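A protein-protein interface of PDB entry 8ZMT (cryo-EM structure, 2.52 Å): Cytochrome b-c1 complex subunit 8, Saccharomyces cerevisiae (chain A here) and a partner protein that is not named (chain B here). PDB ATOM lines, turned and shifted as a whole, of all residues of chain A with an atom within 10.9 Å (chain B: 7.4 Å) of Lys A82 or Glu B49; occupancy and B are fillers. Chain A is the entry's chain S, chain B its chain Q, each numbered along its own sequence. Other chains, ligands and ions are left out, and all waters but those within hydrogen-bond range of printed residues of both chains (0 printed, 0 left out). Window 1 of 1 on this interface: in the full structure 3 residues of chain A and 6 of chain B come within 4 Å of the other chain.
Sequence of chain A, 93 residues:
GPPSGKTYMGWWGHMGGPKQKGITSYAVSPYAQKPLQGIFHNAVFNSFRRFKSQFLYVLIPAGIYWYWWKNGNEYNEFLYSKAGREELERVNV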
ATOM      1  N   TYR A  75     -36.576  26.678  15.137  1.00  0.00           N
ATOM      2  CA  TYR A  75     -36.080  25.804  14.083  1.00  0.00           C
ATOM      3  C   TYR A  75     -35.542  26.607  12.907  1.00  0.00           C
ATOM      4  O   TYR A  75     -34.621  26.161  12.216  1.00  0.00           O
ATOM      5  CB  TYR A  75     -37.194  24.858  13.637  1.00  0.00           C
ATOM      6  CG  TYR A  75     -36.823  23.898  12.537  1.00  0.00           C
ATOM      7  CD1 TYR A  75     -35.756  23.025  12.682  1.00  0.00           C
ATOM      8  CD2 TYR A  75     -37.550  23.856  11.358  1.00  0.00           C
ATOM      9  CE1 TYR A  75     -35.420  22.143  11.678  1.00  0.00           C
ATOM     10  CE2 TYR A  75     -37.222  22.979  10.351  1.00  0.00           C
ATOM     11  CZ  TYR A  75     -36.159  22.127  10.517  1.00  0.00           C
ATOM     12  OH  TYR A  75     -35.832  21.253   9.511  1.00  0.00           O
ATOM     13  N   ASN A  76     -36.102  27.794  12.670  1.00  0.00           N
ATOM     14  CA  ASN A  76     -35.584  28.672  11.627  1.00  0.00           C
ATOM     15  C   ASN A  76     -34.244  29.273  12.036  1.00  0.00           C
ATOM     16  O   ASN A  76     -33.392  29.544  11.184  1.00  0.00           O
ATOM     17  CB  ASN A  76     -36.607  29.766  11.324  1.00  0.00           C
ATOM     18  CG  ASN A  76     -36.149  30.719  10.247  1.00  0.00           C
ATOM     19  OD1 ASN A  76     -36.300  30.452   9.061  1.00  0.00           O
ATOM     20  ND2 ASN A  76     -35.601  31.849  10.657  1.00  0.00           N
ATOM     21  N   GLU A  77     -34.039  29.484  13.336  1.00  0.00           N
ATOM     22  CA  GLU A  77     -32.759  29.987  13.818  1.00  0.00           C
ATOM     23  C   GLU A  77     -31.664  28.937  13.713  1.00  0.00           C
ATOM     24  O   GLU A  77     -30.489  29.282  13.557  1.00  0.00           O
ATOM     25  CB  GLU A  77     -32.888  30.456  15.263  1.00  0.00           C
ATOM     26  CG  GLU A  77     -33.296  31.901  15.413  1.00  0.00           C
ATOM     27  CD  GLU A  77     -33.478  32.302  16.862  1.00  0.00           C
ATOM     28  OE1 GLU A  77     -34.592  32.734  17.228  1.00  0.00           O
ATOM     29  OE2 GLU A  77     -32.507  32.181  17.637  1.00  0.00           O
ATOM     30  N   PHE A  78     -32.022  27.658  13.807  1.00  0.00           N
ATOM     31  CA  PHE A  78     -31.044  26.590  13.660  1.00  0.00           C
ATOM     32  C   PHE A  78     -30.649  26.386  12.205  1.00  0.00           C
ATOM     33  O   PHE A  78     -29.499  26.037  11.925  1.00  0.00           O
ATOM     34  CB  PHE A  78     -31.605  25.298  14.264  1.00  0.00           C
ATOM     35  CG  PHE A  78     -30.831  24.060  13.907  1.00  0.00           C
ATOM     36  CD1 PHE A  78     -29.630  23.779  14.530  1.00  0.00           C
ATOM     37  CD2 PHE A  78     -31.315  23.170  12.962  1.00  0.00           C
ATOM     38  CE1 PHE A  78     -28.916  22.645  14.207  1.00  0.00           C
ATOM     39  CE2 PHE A  78     -30.605  22.038  12.633  1.00  0.00           C
ATOM     40  CZ  PHE A  78     -29.405  21.774  13.259  1.00  0.00           C
ATOM     41  N   LEU A  79     -31.579  26.609  11.273  1.00  0.00           N
ATOM     42  CA  LEU A  79     -31.315  26.322   9.867  1.00  0.00           C
ATOM     43  C   LEU A  79     -30.350  27.319   9.248  1.00  0.00           C
ATOM     44  O   LEU A  79     -29.656  26.991   8.282  1.00  0.00           O
ATOM     45  CB  LEU A  79     -32.622  26.317   9.076  1.00  0.00           C
ATOM     46  CG  LEU A  79     -33.520  25.085   9.151  1.00  0.00           C
ATOM     47  CD1 LEU A  79     -34.732  25.290   8.272  1.00  0.00           C
ATOM     48  CD2 LEU A  79     -32.770  23.835   8.744  1.00  0.00           C
ATOM     49  N   TYR A  80     -30.294  28.539   9.775  1.00  0.00           N
ATOM     50  CA  TYR A  80     -29.441  29.579   9.221  1.00  0.00           C
ATOM     51  C   TYR A  80     -28.211  29.843  10.072  1.00  0.00           C
ATOM     52  O   TYR A  80     -27.505  30.826   9.836  1.00  0.00           O
ATOM     53  CB  TYR A  80     -30.244  30.862   9.024  1.00  0.00           C
ATOM     54  CG  TYR A  80     -31.126  30.800   7.807  1.00  0.00           C
ATOM     55  CD1 TYR A  80     -30.620  31.084   6.550  1.00  0.00           C
ATOM     56  CD2 TYR A  80     -32.459  30.435   7.911  1.00  0.00           C
ATOM     57  CE1 TYR A  80     -31.416  31.018   5.434  1.00  0.00           C
ATOM     58  CE2 TYR A  80     -33.264  30.364   6.798  1.00  0.00           C
ATOM     59  CZ  TYR A  80     -32.736  30.659   5.563  1.00  0.00           C
ATOM     60  OH  TYR A  80     -33.530  30.591   4.446  1.00  0.00           O
ATOM     61  N   SER A  81     -27.934  28.992  11.052  1.00  0.00           N
ATOM     62  CA  SER A  81     -26.686  29.062  11.795  1.00  0.00           C
ATOM     63  C   SER A  81     -25.630  28.243  11.058  1.00  0.00           C
ATOM     64  O   SER A  81     -25.842  27.770   9.939  1.00  0.00           O
ATOM     65  CB  SER A  81     -26.895  28.588  13.229  1.00  0.00           C
ATOM     66  OG  SER A  81     -27.123  27.194  13.279  1.00  0.00           O
ATOM     67  N   LYS A  82     -24.467  28.063  11.683  1.00  0.00           N
ATOM     68  CA  LYS A  82     -23.396  27.309  11.045  1.00  0.00           C
ATOM     69  C   LYS A  82     -23.617  25.808  11.178  1.00  0.00           C
ATOM     70  O   LYS A  82     -23.302  25.047  10.258  1.00  0.00           O
ATOM     71  CB  LYS A  82     -22.048  27.713  11.642  1.00  0.00           C
ATOM     72  CG  LYS A  82     -20.846  27.118  10.933  1.00  0.00           C
ATOM     73  CD  LYS A  82     -19.558  27.389  11.687  1.00  0.00           C
ATOM     74  CE  LYS A  82     -19.138  28.838  11.558  1.00  0.00           C
ATOM     75  NZ  LYS A  82     -17.764  29.051  12.084  1.00  0.00           N
ATOM     76  N   ALA A  83     -24.172  25.370  12.309  1.00  0.00           N
ATOM     77  CA  ALA A  83     -24.384  23.948  12.545  1.00  0.00           C
ATOM     78  C   ALA A  83     -25.526  23.373  11.719  1.00  0.00           C
ATOM     79  O   ALA A  83     -25.600  22.151  11.558  1.00  0.00           O
ATOM     80  CB  ALA A  83     -24.648  23.703  14.029  1.00  0.00           C
ATOM     81  N   GLY A  84     -26.413  24.211  11.196  1.00  0.00           N
ATOM     82  CA  GLY A  84     -27.552  23.722  10.449  1.00  0.00           C
ATOM     83  C   GLY A  84     -27.449  23.936   8.955  1.00  0.00           C
ATOM     84  O   GLY A  84     -28.438  24.290   8.310  1.00  0.00           O
ATOM     85  N   ARG A  85     -26.262  23.729   8.388  1.00  0.00           N
ATOM     86  CA  ARG A  85     -26.040  24.032   6.982  1.00  0.00           C
ATOM     87  C   ARG A  85     -26.346  22.869   6.047  1.00  0.00           C
ATOM     88  O   ARG A  85     -26.805  23.107   4.924  1.00  0.00           O
ATOM     89  CB  ARG A  85     -24.597  24.494   6.768  1.00  0.00           C
ATOM     90  CG  ARG A  85     -24.408  25.359   5.539  1.00  0.00           C
ATOM     91  CD  ARG A  85     -22.942  25.657   5.309  1.00  0.00           C
ATOM     92  NE  ARG A  85     -22.138  24.440   5.288  1.00  0.00           N
ATOM     93  CZ  ARG A  85     -21.922  23.706   4.203  1.00  0.00           C
ATOM     94  NH1 ARG A  85     -22.450  24.061   3.042  1.00  0.00           N
ATOM     95  NH2 ARG A  85     -21.176  22.613   4.281  1.00  0.00           N
ATOM     96  N   GLU A  86     -26.108  21.625   6.465  1.00  0.00           N
ATOM     97  CA  GLU A  86     -26.486  20.493   5.624  1.00  0.00           C
ATOM     98  C   GLU A  86     -27.947  20.100   5.778  1.00  0.00           C
ATOM     99  O   GLU A  86     -28.451  19.313   4.975  1.00  0.00           O
ATOM    100  CB  GLU A  86     -25.588  19.283   5.883  1.00  0.00           C
ATOM    101  CG  GLU A  86     -24.313  19.577   6.631  1.00  0.00           C
ATOM    102  CD  GLU A  86     -23.216  20.056   5.690  1.00  0.00           C
ATOM    103  OE1 GLU A  86     -23.425  20.022   4.457  1.00  0.00           O
ATOM    104  OE2 GLU A  86     -22.140  20.460   6.178  1.00  0.00           O
ATOM    105  N   GLU A  87     -28.641  20.596   6.798  1.00  0.00           N
ATOM    106  CA  GLU A  87     -30.081  20.388   6.800  1.00  0.00           C
ATOM    107  C   GLU A  87     -30.780  21.428   5.932  1.00  0.00           C
ATOM    108  O   GLU A  87     -31.846  21.153   5.372  1.00  0.00           O
ATOM    109  CB  GLU A  87     -30.623  20.406   8.231  1.00  0.00           C
ATOM    110  CG  GLU A  87     -32.080  19.964   8.342  1.00  0.00           C
ATOM    111  CD  GLU A  87     -32.503  19.623   9.751  1.00  0.00           C
ATOM    112  OE1 GLU A  87     -31.628  19.535  10.634  1.00  0.00           O
ATOM    113  OE2 GLU A  87     -33.718  19.445   9.974  1.00  0.00           O
ATOM    114  N   LEU A  88     -30.166  22.602   5.762  1.00  0.00           N
ATOM    115  CA  LEU A  88     -30.762  23.656   4.946  1.00  0.00           C
ATOM    116  C   LEU A  88     -30.763  23.295   3.468  1.00  0.00           C
ATOM    117  O   LEU A  88     -31.667  23.701   2.733  1.00  0.00           O
ATOM    118  CB  LEU A  88     -30.015  24.971   5.180  1.00  0.00           C
ATOM    119  CG  LEU A  88     -30.466  26.234   4.449  1.00  0.00           C
ATOM    120  CD1 LEU A  88     -31.919  26.541   4.738  1.00  0.00           C
ATOM    121  CD2 LEU A  88     -29.588  27.417   4.811  1.00  0.00           C
ATOM    122  N   GLU A  89     -29.779  22.517   3.017  1.00  0.00           N
ATOM    123  CA  GLU A  89     -29.716  22.163   1.603  1.00  0.00           C
ATOM    124  C   GLU A  89     -30.744  21.101   1.229  1.00  0.00           C
ATOM    125  O   GLU A  89     -31.136  21.012   0.062  1.00  0.00           O
ATOM    126  CB  GLU A  89     -28.301  21.702   1.239  1.00  0.00           C
ATOM    127  CG  GLU A  89     -27.754  20.548   2.071  1.00  0.00           C
ATOM    128  CD  GLU A  89     -28.105  19.175   1.519  1.00  0.00           C
ATOM    129  OE1 GLU A  89     -28.409  19.079   0.313  1.00  0.00           O
ATOM    130  OE2 GLU A  89     -28.095  18.196   2.295  1.00  0.00           O
ATOM    131  N   CYS B  29     -10.908  29.495  16.338  1.00  0.00           N
ATOM    132  CA  CYS B  29     -11.570  29.399  15.043  1.00  0.00           C
ATOM    133  C   CYS B  29     -10.660  29.901  13.934  1.00  0.00           C
ATOM    134  O   CYS B  29     -10.635  29.334  12.838  1.00  0.00           O
ATOM    135  CB  CYS B  29     -12.878  30.196  15.057  1.00  0.00           C
ATOM    136  SG  CYS B  29     -13.838  30.181  13.506  1.00  0.00           S
ATOM    137  N   ARG B  32      -8.022  27.420  12.436  1.00  0.00           N
ATOM    138  CA  ARG B  32      -8.508  26.450  11.461  1.00  0.00           C
ATOM    139  C   ARG B  32      -8.678  27.083  10.086  1.00  0.00           C
ATOM    140  O   ARG B  32      -8.405  26.444   9.064  1.00  0.00           O
ATOM    141  CB  ARG B  32      -9.832  25.853  11.933  1.00  0.00           C
ATOM    142  CG  ARG B  32      -9.697  24.827  13.034  1.00  0.00           C
ATOM    143  CD  ARG B  32     -10.994  24.060  13.224  1.00  0.00           C
ATOM    144  NE  ARG B  32     -11.923  24.757  14.107  1.00  0.00           N
ATOM    145  CZ  ARG B  32     -12.962  25.470  13.687  1.00  0.00           C
ATOM    146  NH1 ARG B  32     -13.752  26.069  14.566  1.00  0.00           N
ATOM    147  NH2 ARG B  32     -13.212  25.584  12.392  1.00  0.00           N
ATOM    148  N   VAL B  33      -9.128  28.338  10.044  1.00  0.00           N
ATOM    149  CA  VAL B  33      -9.316  29.029   8.772  1.00  0.00           C
ATOM    150  C   VAL B  33      -7.969  29.376   8.153  1.00  0.00           C
ATOM    151  O   VAL B  33      -7.817  29.354   6.926  1.00  0.00           O
ATOM    152  CB  VAL B  33     -10.204  30.273   8.986  1.00  0.00           C
ATOM    153  CG1 VAL B  33     -10.473  31.007   7.683  1.00  0.00           C
ATOM    154  CG2 VAL B  33     -11.511  29.865   9.623  1.00  0.00           C
ATOM    155  N   LYS B  34      -6.961  29.649   8.985  1.00  0.00           N
ATOM    156  CA  LYS B  34      -5.630  29.959   8.477  1.00  0.00           C
ATOM    157  C   LYS B  34      -4.967  28.753   7.824  1.00  0.00           C
ATOM    158  O   LYS B  34      -4.345  28.896   6.765  1.00  0.00           O
ATOM    159  CB  LYS B  34      -4.744  30.491   9.604  1.00  0.00           C
ATOM    160  CG  LYS B  34      -3.372  30.931   9.135  1.00  0.00           C
ATOM    161  CD  LYS B  34      -2.529  31.503  10.255  1.00  0.00           C
ATOM    162  CE  LYS B  34      -1.163  31.902   9.726  1.00  0.00           C
ATOM    163  NZ  LYS B  34      -0.288  32.468  10.782  1.00  0.00           N
ATOM    164  N   GLN B  36      -6.609  26.038   6.497  1.00  0.00           N
ATOM    165  CA  GLN B  36      -7.336  25.518   5.345  1.00  0.00           C
ATOM    166  C   GLN B  36      -7.257  26.438   4.129  1.00  0.00           C
ATOM    167  O   GLN B  36      -7.620  26.029   3.024  1.00  0.00           O
ATOM    168  CB  GLN B  36      -8.799  25.234   5.708  1.00  0.00           C
ATOM    169  CG  GLN B  36      -9.659  26.440   5.984  1.00  0.00           C
ATOM    170  CD  GLN B  36     -11.073  26.047   6.376  1.00  0.00           C
ATOM    171  OE1 GLN B  36     -11.417  24.865   6.404  1.00  0.00           O
ATOM    172  NE2 GLN B  36     -11.899  27.038   6.676  1.00  0.00           N
ATOM    173  N   GLN B  37      -6.803  27.680   4.300  1.00  0.00           N
ATOM    174  CA  GLN B  37      -6.646  28.539   3.130  1.00  0.00           C
ATOM    175  C   GLN B  37      -5.192  28.779   2.741  1.00  0.00           C
ATOM    176  O   GLN B  37      -4.936  29.468   1.748  1.00  0.00           O
ATOM    177  CB  GLN B  37      -7.352  29.882   3.340  1.00  0.00           C
ATOM    178  CG  GLN B  37      -6.651  30.861   4.256  1.00  0.00           C
ATOM    179  CD  GLN B  37      -7.491  32.094   4.518  1.00  0.00           C
ATOM    180  OE1 GLN B  37      -8.573  32.255   3.952  1.00  0.00           O
ATOM    181  NE2 GLN B  37      -6.999  32.971   5.381  1.00  0.00           N
ATOM    182  N   LEU B  45     -13.088  24.560  -3.376  1.00  0.00           N
ATOM    183  CA  LEU B  45     -13.972  24.196  -2.282  1.00  0.00           C
ATOM    184  C   LEU B  45     -15.382  24.730  -2.505  1.00  0.00           C
ATOM    185  O   LEU B  45     -15.587  25.790  -3.105  1.00  0.00           O
ATOM    186  CB  LEU B  45     -13.421  24.695  -0.947  1.00  0.00           C
ATOM    187  CG  LEU B  45     -12.076  24.073  -0.575  1.00  0.00           C
ATOM    188  CD1 LEU B  45     -11.382  24.859   0.523  1.00  0.00           C
ATOM    189  CD2 LEU B  45     -12.267  22.621  -0.167  1.00  0.00           C
ATOM    190  N   HIS B  47     -17.561  25.371   0.047  1.00  0.00           N
ATOM    191  CA  HIS B  47     -17.941  26.289   1.115  1.00  0.00           C
ATOM    192  C   HIS B  47     -16.694  26.666   1.899  1.00  0.00           C
ATOM    193  O   HIS B  47     -16.079  25.806   2.540  1.00  0.00           O
ATOM    194  CB  HIS B  47     -18.997  25.660   2.026  1.00  0.00           C
ATOM    195  CG  HIS B  47     -19.061  26.277   3.388  1.00  0.00           C
ATOM    196  ND1 HIS B  47     -18.489  25.693   4.496  1.00  0.00           N
ATOM    197  CD2 HIS B  47     -19.625  27.431   3.819  1.00  0.00           C
ATOM    198  CE1 HIS B  47     -18.706  26.456   5.553  1.00  0.00           C
ATOM    199  NE2 HIS B  47     -19.390  27.518   5.169  1.00  0.00           N
ATOM    200  N   LYS B  48     -16.315  27.936   1.831  1.00  0.00           N
ATOM    201  CA  LYS B  48     -15.227  28.460   2.643  1.00  0.00           C
ATOM    202  C   LYS B  48     -15.776  28.868   4.004  1.00  0.00           C
ATOM    203  O   LYS B  48     -16.803  29.551   4.087  1.00  0.00           O
ATOM    204  CB  LYS B  48     -14.559  29.658   1.960  1.00  0.00           C
ATOM    205  CG  LYS B  48     -13.902  29.349   0.625  1.00  0.00           C
ATOM    206  CD  LYS B  48     -12.702  28.419   0.761  1.00  0.00           C
ATOM    207  CE  LYS B  48     -11.497  29.129   1.368  1.00  0.00           C
ATOM    208  NZ  LYS B  48     -10.281  28.265   1.401  1.00  0.00           N
ATOM    209  N   GLU B  49     -15.091  28.453   5.064  1.00  0.00           N
ATOM    210  CA  GLU B  49     -15.534  28.727   6.422  1.00  0.00           C
ATOM    211  C   GLU B  49     -14.889  30.002   6.950  1.00  0.00           C
ATOM    212  O   GLU B  49     -13.680  30.203   6.812  1.00  0.00           O
ATOM    213  CB  GLU B  49     -15.196  27.553   7.345  1.00  0.00           C
ATOM    214  CG  GLU B  49     -15.638  27.744   8.788  1.00  0.00           C
ATOM    215  CD  GLU B  49     -14.998  26.754   9.745  1.00  0.00           C
ATOM    216  OE1 GLU B  49     -14.244  25.875   9.280  1.00  0.00           O
ATOM    217  OE2 GLU B  49     -15.252  26.853  10.964  1.00  0.00           O
ATOM    218  N   ASP B  50     -15.704  30.861   7.554  1.00  0.00           N
ATOM    219  CA  ASP B  50     -15.242  32.069   8.224  1.00  0.00           C
ATOM    220  C   ASP B  50     -15.614  32.004   9.703  1.00  0.00           C
ATOM    221  O   ASP B  50     -16.245  31.054  10.168  1.00  0.00           O
ATOM    222  CB  ASP B  50     -15.823  33.319   7.561  1.00  0.00           C
ATOM    223  CG  ASP B  50     -17.323  33.406   7.697  1.00  0.00           C
ATOM    224  OD1 ASP B  50     -17.900  32.592   8.447  1.00  0.00           O
ATOM    225  OD2 ASP B  50     -17.929  34.286   7.052  1.00  0.00           O
ATOM    226  N   CYS B  51     -15.219  33.030  10.449  1.00  0.00           N
ATOM    227  CA  CYS B  51     -15.465  33.100  11.883  1.00  0.00           C
ATOM    228  C   CYS B  51     -16.301  34.319  12.240  1.00  0.00           C
ATOM    229  O   CYS B  51     -15.977  35.062  13.166  1.00  0.00           O
ATOM    230  CB  CYS B  51     -14.155  33.110  12.664  1.00  0.00           C
ATOM    231  SG  CYS B  51     -13.095  31.695  12.362  1.00  0.00           S
ATOM    232  N   VAL B  52     -17.388  34.540  11.503  1.00  0.00           N
ATOM    233  CA  VAL B  52     -18.245  35.689  11.775  1.00  0.00           C
ATOM    234  C   VAL B  52     -19.077  35.456  13.034  1.00  0.00           C
ATOM    235  O   VAL B  52     -19.250  36.367  13.852  1.00  0.00           O
ATOM    236  CB  VAL B  52     -19.120  35.992  10.543  1.00  0.00           C
ATOM    237  CG1 VAL B  52     -20.157  37.055  10.838  1.00  0.00           C
ATOM    238  CG2 VAL B  52     -18.252  36.439   9.390  1.00  0.00           C
ATOM    239  N   GLU B  53     -19.566  34.225  13.231  1.00  0.00           N
ATOM    240  CA  GLU B  53     -20.430  33.936  14.375  1.00  0.00           C
ATOM    241  C   GLU B  53     -19.665  33.994  15.691  1.00  0.00           C
ATOM    242  O   GLU B  53     -20.221  34.391  16.719  1.00  0.00           O
ATOM    243  CB  GLU B  53     -21.082  32.567  14.225  1.00  0.00           C
ATOM    244  CG  GLU B  53     -22.085  32.457  13.105  1.00  0.00           C
ATOM    245  CD  GLU B  53     -22.772  31.108  13.088  1.00  0.00           C
ATOM    246  OE1 GLU B  53     -22.414  30.247  13.919  1.00  0.00           O
ATOM    247  OE2 GLU B  53     -23.661  30.904  12.237  1.00  0.00           O
ATOM    248  N   GLU B  54     -18.397  33.589  15.681  1.00  0.00           N
ATOM    249  CA  GLU B  54     -17.584  33.694  16.885  1.00  0.00           C
ATOM    250  C   GLU B  54     -17.204  35.141  17.159  1.00  0.00           C
ATOM    251  O   GLU B  54     -16.966  35.521  18.310  1.00  0.00           O
ATOM    252  CB  GLU B  54     -16.340  32.818  16.749  1.00  0.00           C
ATOM    253  CG  GLU B  54     -16.624  31.326  16.790  1.00  0.00           C
ATOM    254  CD  GLU B  54     -16.971  30.748  15.430  1.00  0.00           C
ATOM    255  OE1 GLU B  54     -17.225  29.529  15.347  1.00  0.00           O
ATOM    256  OE2 GLU B  54     -16.994  31.509  14.444  1.00  0.00           O
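O of Phe A78 lies within hydrogen-bond range of OG of Ser A81. The guanidinium group of Arg A85 lies within salt-bridge range of the side-chain carboxylate of Glu A86. The side-chain sulfur of Cys B29 forms a disulfide with the side-chain sulfur of Cys B51 (2.0 Å). The side-chain carboxylate (OE2) of Glu B49 lies within salt-bridge range of the guanidinium group (NH2) of Arg B32 (2.8 Å).
The backbone NH of Lys A82 is in hydrogen-bond range of the side-chain carboxylate of Glu B53 (3.0 Å). NZ of Lys A82 lies within hydrogen-bond range of O of Asp B50 (3.2 Å). The side-chain carboxylate (OE1) of Glu B54 is in salt-bridge range of the side-chain amino group (NZ) of Lys A82, 3.3 Å away. NZ of Lys A82 lies within salt-bridge range of OE2 of Glu B49, at 3.5 Å.
Hydrophobic or aromatic side chains of chain B within 4 Å of the printed part of chain A: His B47. Along chain B the printed residues that touch a printed residue of chain A span positions 47 to 54. Of the 15 printed residues of chain A, 3 touch a printed residue of chain B. Among the printed residues, Asp or Glu carboxylates within 4 Å of a Lys or Arg side-chain nitrogen of the other chain: Lys A82 with Glu B49 (3.5 Å) and Lys A82 with Glu B54 (3.3 Å).
C of Ser A81 touches OE2 of Glu B53, 3.5 Å away. Arg A85 touches His B47 (CZ to CG, 3.9 Å).
Lys A82 touches just these residues of chain B: Glu B49 (3.5 Å), Asp B50 (3.2 Å), Glu B53 (3.0 Å) and Glu B54 (3.3 Å). Of chain A, only Lys A82 (3.5 Å) comes within 4 Å of Glu B49. No residue of chain A comes within 4 Å of Val B33. His B47 touches just one residue of chain A: Arg A85 (3.9 Å). Of the printed residues of chain A, Asp B50 touches Lys A82. No residue of chain A comes within 4 Å of Cys B51. Printed residues of chain B within 4 Å of Ser A81: Glu B53. Printed residues of chain B within 4 Å of Arg A85: His B47 (3.9 Å). Of the printed residues of chain A, Glu B53 touches Ser A81 (3.5 Å) and Lys A82 (3.0 Å). Of the printed residues of chain A, Glu B54 touches Lys A82 (3.3 Å). Glu A89 touches none of the printed residues of chain B. Ala A83 touches none of the printed residues of chain B. The nearest residue of chain B that does not touch Lys A82 is Cys B29 (4.3 Å).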
